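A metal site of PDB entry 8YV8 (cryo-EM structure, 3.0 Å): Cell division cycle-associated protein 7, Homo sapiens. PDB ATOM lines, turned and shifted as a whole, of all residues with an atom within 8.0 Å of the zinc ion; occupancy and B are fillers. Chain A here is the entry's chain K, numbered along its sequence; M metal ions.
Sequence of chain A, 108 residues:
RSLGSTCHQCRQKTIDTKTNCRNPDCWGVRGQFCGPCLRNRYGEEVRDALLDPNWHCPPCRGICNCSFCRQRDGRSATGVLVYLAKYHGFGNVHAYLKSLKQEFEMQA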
ATOM      1  N   ASN A  20      17.457  31.638  16.275  1.00  0.00           N
ATOM      2  CA  ASN A  20      17.072  30.519  17.121  1.00  0.00           C
ATOM      3  C   ASN A  20      15.844  30.884  17.938  1.00  0.00           C
ATOM      4  O   ASN A  20      15.590  32.058  18.230  1.00  0.00           O
ATOM      5  CB  ASN A  20      18.215  30.109  18.050  1.00  0.00           C
ATOM      6  CG  ASN A  20      18.038  28.708  18.606  1.00  0.00           C
ATOM      7  OD1 ASN A  20      16.989  28.080  18.422  1.00  0.00           O
ATOM      8  ND2 ASN A  20      19.060  28.208  19.290  1.00  0.00           N
ATOM      9  N   CYS A  21      15.076  29.862  18.311  1.00  0.00           N
ATOM     10  CA  CYS A  21      13.864  30.041  19.092  1.00  0.00           C
ATOM     11  C   CYS A  21      14.198  29.855  20.573  1.00  0.00           C
ATOM     12  O   CYS A  21      14.761  28.821  20.958  1.00  0.00           O
ATOM     13  CB  CYS A  21      12.776  29.052  18.661  1.00  0.00           C
ATOM     14  SG  CYS A  21      11.154  29.352  19.388  1.00  0.00           S
ATOM     15  N   ARG A  22      13.844  30.844  21.389  1.00  0.00           N
ATOM     16  CA  ARG A  22      14.120  30.824  22.815  1.00  0.00           C
ATOM     17  C   ARG A  22      12.959  30.297  23.636  1.00  0.00           C
ATOM     18  O   ARG A  22      13.016  30.318  24.870  1.00  0.00           O
ATOM     19  CB  ARG A  22      14.511  32.237  23.305  1.00  0.00           C
ATOM     20  N   ASN A  23      11.906  29.826  22.984  1.00  0.00           N
ATOM     21  CA  ASN A  23      10.771  29.239  23.700  1.00  0.00           C
ATOM     22  C   ASN A  23      11.202  27.940  24.354  1.00  0.00           C
ATOM     23  O   ASN A  23      11.693  27.038  23.663  1.00  0.00           O
ATOM     24  CB  ASN A  23       9.610  29.009  22.736  1.00  0.00           C
ATOM     25  CG  ASN A  23       8.292  28.785  23.457  1.00  0.00           C
ATOM     26  OD1 ASN A  23       8.254  28.354  24.614  1.00  0.00           O
ATOM     27  ND2 ASN A  23       7.190  29.078  22.776  1.00  0.00           N
ATOM     28  N   PRO A  24      11.059  27.794  25.679  1.00  0.00           N
ATOM     29  CA  PRO A  24      11.361  26.492  26.298  1.00  0.00           C
ATOM     30  C   PRO A  24      10.496  25.366  25.752  1.00  0.00           C
ATOM     31  O   PRO A  24      10.966  24.229  25.671  1.00  0.00           O
ATOM     32  CB  PRO A  24      11.091  26.750  27.787  1.00  0.00           C
ATOM     33  CG  PRO A  24      10.235  27.984  27.835  1.00  0.00           C
ATOM     34  CD  PRO A  24      10.664  28.810  26.661  1.00  0.00           C
ATOM     35  N   ASP A  25       9.251  25.654  25.383  1.00  0.00           N
ATOM     36  CA  ASP A  25       8.370  24.645  24.799  1.00  0.00           C
ATOM     37  C   ASP A  25       8.635  24.405  23.327  1.00  0.00           C
ATOM     38  O   ASP A  25       8.063  23.468  22.751  1.00  0.00           O
ATOM     39  CB  ASP A  25       6.905  25.048  24.999  1.00  0.00           C
ATOM     40  CG  ASP A  25       6.561  25.288  26.456  1.00  0.00           C
ATOM     41  OD1 ASP A  25       7.067  24.537  27.318  1.00  0.00           O
ATOM     42  OD2 ASP A  25       5.783  26.229  26.739  1.00  0.00           O
ATOM     43  N   CYS A  26       9.482  25.213  22.693  1.00  0.00           N
ATOM     44  CA  CYS A  26       9.817  25.005  21.290  1.00  0.00           C
ATOM     45  C   CYS A  26      10.606  23.715  21.119  1.00  0.00           C
ATOM     46  O   CYS A  26      11.439  23.365  21.958  1.00  0.00           O
ATOM     47  CB  CYS A  26      10.619  26.187  20.744  1.00  0.00           C
ATOM     48  SG  CYS A  26      11.188  25.990  19.041  1.00  0.00           S
ATOM     49  N   TRP A  27      10.332  23.002  20.034  1.00  0.00           N
ATOM     50  CA  TRP A  27      10.987  21.744  19.753  1.00  0.00           C
ATOM     51  C   TRP A  27      11.396  21.702  18.284  1.00  0.00           C
ATOM     52  O   TRP A  27      10.793  22.366  17.433  1.00  0.00           O
ATOM     53  CB  TRP A  27      10.076  20.546  20.076  1.00  0.00           C
ATOM     54  CG  TRP A  27       8.631  20.793  19.769  1.00  0.00           C
ATOM     55  CD1 TRP A  27       7.669  21.206  20.648  1.00  0.00           C
ATOM     56  CD2 TRP A  27       7.979  20.640  18.509  1.00  0.00           C
ATOM     57  NE1 TRP A  27       6.463  21.319  20.008  1.00  0.00           N
ATOM     58  CE2 TRP A  27       6.621  20.983  18.687  1.00  0.00           C
ATOM     59  CE3 TRP A  27       8.410  20.266  17.231  1.00  0.00           C
ATOM     60  CZ2 TRP A  27       5.700  20.942  17.652  1.00  0.00           C
ATOM     61  CZ3 TRP A  27       7.486  20.221  16.205  1.00  0.00           C
ATOM     62  CH2 TRP A  27       6.143  20.566  16.422  1.00  0.00           C
ATOM     63  N   GLY A  28      12.425  20.909  17.996  1.00  0.00           N
ATOM     64  CA  GLY A  28      12.891  20.738  16.641  1.00  0.00           C
ATOM     65  C   GLY A  28      13.700  21.918  16.131  1.00  0.00           C
ATOM     66  O   GLY A  28      14.072  22.830  16.866  1.00  0.00           O
ATOM     67  N   VAL A  29      13.973  21.867  14.827  1.00  0.00           N
ATOM     68  CA  VAL A  29      14.760  22.896  14.159  1.00  0.00           C
ATOM     69  C   VAL A  29      13.879  24.029  13.638  1.00  0.00           C
ATOM     70  O   VAL A  29      14.400  25.081  13.228  1.00  0.00           O
ATOM     71  CB  VAL A  29      15.604  22.222  13.057  1.00  0.00           C
ATOM     72  CG1 VAL A  29      16.351  23.228  12.186  1.00  0.00           C
ATOM     73  CG2 VAL A  29      16.579  21.237  13.678  1.00  0.00           C
ATOM     74  N   ARG A  30      12.548  23.883  13.710  1.00  0.00           N
ATOM     75  CA  ARG A  30      11.622  24.869  13.184  1.00  0.00           C
ATOM     76  C   ARG A  30      11.830  26.272  13.744  1.00  0.00           C
ATOM     77  O   ARG A  30      11.210  27.218  13.248  1.00  0.00           O
ATOM     78  CB  ARG A  30      10.178  24.412  13.443  1.00  0.00           C
ATOM     79  CG  ARG A  30       9.820  24.281  14.917  1.00  0.00           C
ATOM     80  CD  ARG A  30       9.032  25.485  15.425  1.00  0.00           C
ATOM     81  NE  ARG A  30       8.656  25.322  16.824  1.00  0.00           N
ATOM     82  CZ  ARG A  30       8.101  26.269  17.567  1.00  0.00           C
ATOM     83  NH1 ARG A  30       7.853  27.472  17.084  1.00  0.00           N
ATOM     84  NH2 ARG A  30       7.776  26.008  18.831  1.00  0.00           N
ATOM     85  N   GLY A  31      12.670  26.432  14.765  1.00  0.00           N
ATOM     86  CA  GLY A  31      13.025  27.736  15.268  1.00  0.00           C
ATOM     87  C   GLY A  31      14.133  28.432  14.518  1.00  0.00           C
ATOM     88  O   GLY A  31      14.560  29.511  14.921  1.00  0.00           O
ATOM     89  N   GLN A  32      14.605  27.845  13.417  1.00  0.00           N
ATOM     90  CA  GLN A  32      15.711  28.401  12.644  1.00  0.00           C
ATOM     91  C   GLN A  32      15.181  28.993  11.338  1.00  0.00           C
ATOM     92  O   GLN A  32      14.484  28.310  10.585  1.00  0.00           O
ATOM     93  CB  GLN A  32      16.755  27.332  12.343  1.00  0.00           C
ATOM     94  CG  GLN A  32      17.449  26.784  13.585  1.00  0.00           C
ATOM     95  CD  GLN A  32      18.679  25.972  13.245  1.00  0.00           C
ATOM     96  OE1 GLN A  32      18.857  25.531  12.104  1.00  0.00           O
ATOM     97  NE2 GLN A  32      19.542  25.770  14.231  1.00  0.00           N
ATOM     98  N   PHE A  33      15.516  30.257  11.086  1.00  0.00           N
ATOM     99  CA  PHE A  33      15.118  30.950   9.876  1.00  0.00           C
ATOM    100  C   PHE A  33      16.305  31.700   9.298  1.00  0.00           C
ATOM    101  O   PHE A  33      17.176  32.158  10.043  1.00  0.00           O
ATOM    102  CB  PHE A  33      13.973  31.927  10.130  1.00  0.00           C
ATOM    103  CG  PHE A  33      12.616  31.302  10.115  1.00  0.00           C
ATOM    104  CD1 PHE A  33      12.156  30.591  11.211  1.00  0.00           C
ATOM    105  CD2 PHE A  33      11.790  31.419   9.005  1.00  0.00           C
ATOM    106  CE1 PHE A  33      10.910  30.009  11.204  1.00  0.00           C
ATOM    107  CE2 PHE A  33      10.547  30.840   8.990  1.00  0.00           C
ATOM    108  CZ  PHE A  33      10.095  30.134  10.091  1.00  0.00           C
ATOM    109  N   TRP A  55      12.836  37.091  21.780  1.00  0.00           N
ATOM    110  CA  TRP A  55      12.451  36.842  20.402  1.00  0.00           C
ATOM    111  C   TRP A  55      12.104  35.380  20.200  1.00  0.00           C
ATOM    112  O   TRP A  55      12.836  34.481  20.628  1.00  0.00           O
ATOM    113  CB  TRP A  55      13.574  37.251  19.442  1.00  0.00           C
ATOM    114  CG  TRP A  55      13.177  37.138  18.002  1.00  0.00           C
ATOM    115  CD1 TRP A  55      12.648  38.111  17.220  1.00  0.00           C
ATOM    116  CD2 TRP A  55      13.279  35.968  17.176  1.00  0.00           C
ATOM    117  NE1 TRP A  55      12.411  37.637  15.949  1.00  0.00           N
ATOM    118  CE2 TRP A  55      12.795  36.319  15.902  1.00  0.00           C
ATOM    119  CE3 TRP A  55      13.741  34.664  17.386  1.00  0.00           C
ATOM    120  CZ2 TRP A  55      12.758  35.416  14.843  1.00  0.00           C
ATOM    121  CZ3 TRP A  55      13.704  33.770  16.342  1.00  0.00           C
ATOM    122  CH2 TRP A  55      13.212  34.151  15.077  1.00  0.00           C
ATOM    123  N   HIS A  56      10.977  35.126  19.542  1.00  0.00           N
ATOM    124  CA  HIS A  56      10.495  33.785  19.264  1.00  0.00           C
ATOM    125  C   HIS A  56      10.405  33.577  17.764  1.00  0.00           C
ATOM    126  O   HIS A  56      10.202  34.514  16.998  1.00  0.00           O
ATOM    127  CB  HIS A  56       9.134  33.545  19.919  1.00  0.00           C
ATOM    128  CG  HIS A  56       9.198  33.368  21.402  1.00  0.00           C
ATOM    129  ND1 HIS A  56       9.659  34.350  22.252  1.00  0.00           N
ATOM    130  CD2 HIS A  56       8.856  32.323  22.191  1.00  0.00           C
ATOM    131  CE1 HIS A  56       9.602  33.916  23.492  1.00  0.00           C
ATOM    132  NE2 HIS A  56       9.119  32.688  23.495  1.00  0.00           N
ATOM    133  N   CYS A  57      10.570  32.323  17.343  1.00  0.00           N
ATOM    134  CA  CYS A  57      10.449  31.982  15.938  1.00  0.00           C
ATOM    135  C   CYS A  57       9.016  32.231  15.468  1.00  0.00           C
ATOM    136  O   CYS A  57       8.076  32.091  16.247  1.00  0.00           O
ATOM    137  CB  CYS A  57      10.847  30.531  15.697  1.00  0.00           C
ATOM    138  SG  CYS A  57       9.699  29.329  16.389  1.00  0.00           S
ATOM    139  N   PRO A  58       8.832  32.603  14.202  1.00  0.00           N
ATOM    140  CA  PRO A  58       7.479  32.919  13.705  1.00  0.00           C
ATOM    141  C   PRO A  58       6.480  31.800  13.951  1.00  0.00           C
ATOM    142  O   PRO A  58       5.301  32.086  14.200  1.00  0.00           O
ATOM    143  CB  PRO A  58       7.700  33.172  12.201  1.00  0.00           C
ATOM    144  CG  PRO A  58       9.175  32.954  11.942  1.00  0.00           C
ATOM    145  CD  PRO A  58       9.875  33.007  13.257  1.00  0.00           C
ATOM    146  N   PRO A  59       6.881  30.521  13.881  1.00  0.00           N
ATOM    147  CA  PRO A  59       5.957  29.479  14.352  1.00  0.00           C
ATOM    148  C   PRO A  59       5.558  29.623  15.820  1.00  0.00           C
ATOM    149  O   PRO A  59       4.433  29.265  16.180  1.00  0.00           O
ATOM    150  CB  PRO A  59       6.721  28.177  14.100  1.00  0.00           C
ATOM    151  CG  PRO A  59       7.623  28.499  12.986  1.00  0.00           C
ATOM    152  CD  PRO A  59       8.035  29.916  13.203  1.00  0.00           C
ATOM    153  N   CYS A  60       6.464  30.120  16.670  1.00  0.00           N
ATOM    154  CA  CYS A  60       6.132  30.256  18.090  1.00  0.00           C
ATOM    155  C   CYS A  60       5.023  31.276  18.305  1.00  0.00           C
ATOM    156  O   CYS A  60       4.105  31.050  19.102  1.00  0.00           O
ATOM    157  CB  CYS A  60       7.383  30.634  18.884  1.00  0.00           C
ATOM    158  SG  CYS A  60       8.733  29.437  18.769  1.00  0.00           S
ATOM    159  N   ARG A  61       5.088  32.417  17.608  1.00  0.00           N
ATOM    160  CA  ARG A  61       4.014  33.396  17.706  1.00  0.00           C
ATOM    161  C   ARG A  61       2.799  33.027  16.860  1.00  0.00           C
ATOM    162  O   ARG A  61       1.763  33.696  16.960  1.00  0.00           O
ATOM    163  CB  ARG A  61       4.491  34.792  17.295  1.00  0.00           C
HETATM  164 ZN    ZN M   1      10.163  27.784  18.026  1.00  0.00          ZN
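SG of Cys 60 forms a disulfide with SG of Cys 21, 2.5 Å away. N of Cys 21 sits at hydrogen-bond distance from O of Gly 31 (3.4 Å). SG of Cys 21 lies close to N of Asn 23.
Gly 31 touches the zinc ion. Of the 21 residues printed, 6 come within 4 Å of the zinc ion.
The zinc ion is bound by SG of Cys 57 (2.3 Å), SG of Cys 21 (2.3 Å), SG of Cys 26 (2.3 Å), SG of Cys 60 (2.3 Å) and NH1 of Arg 30 (2.5 Å).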
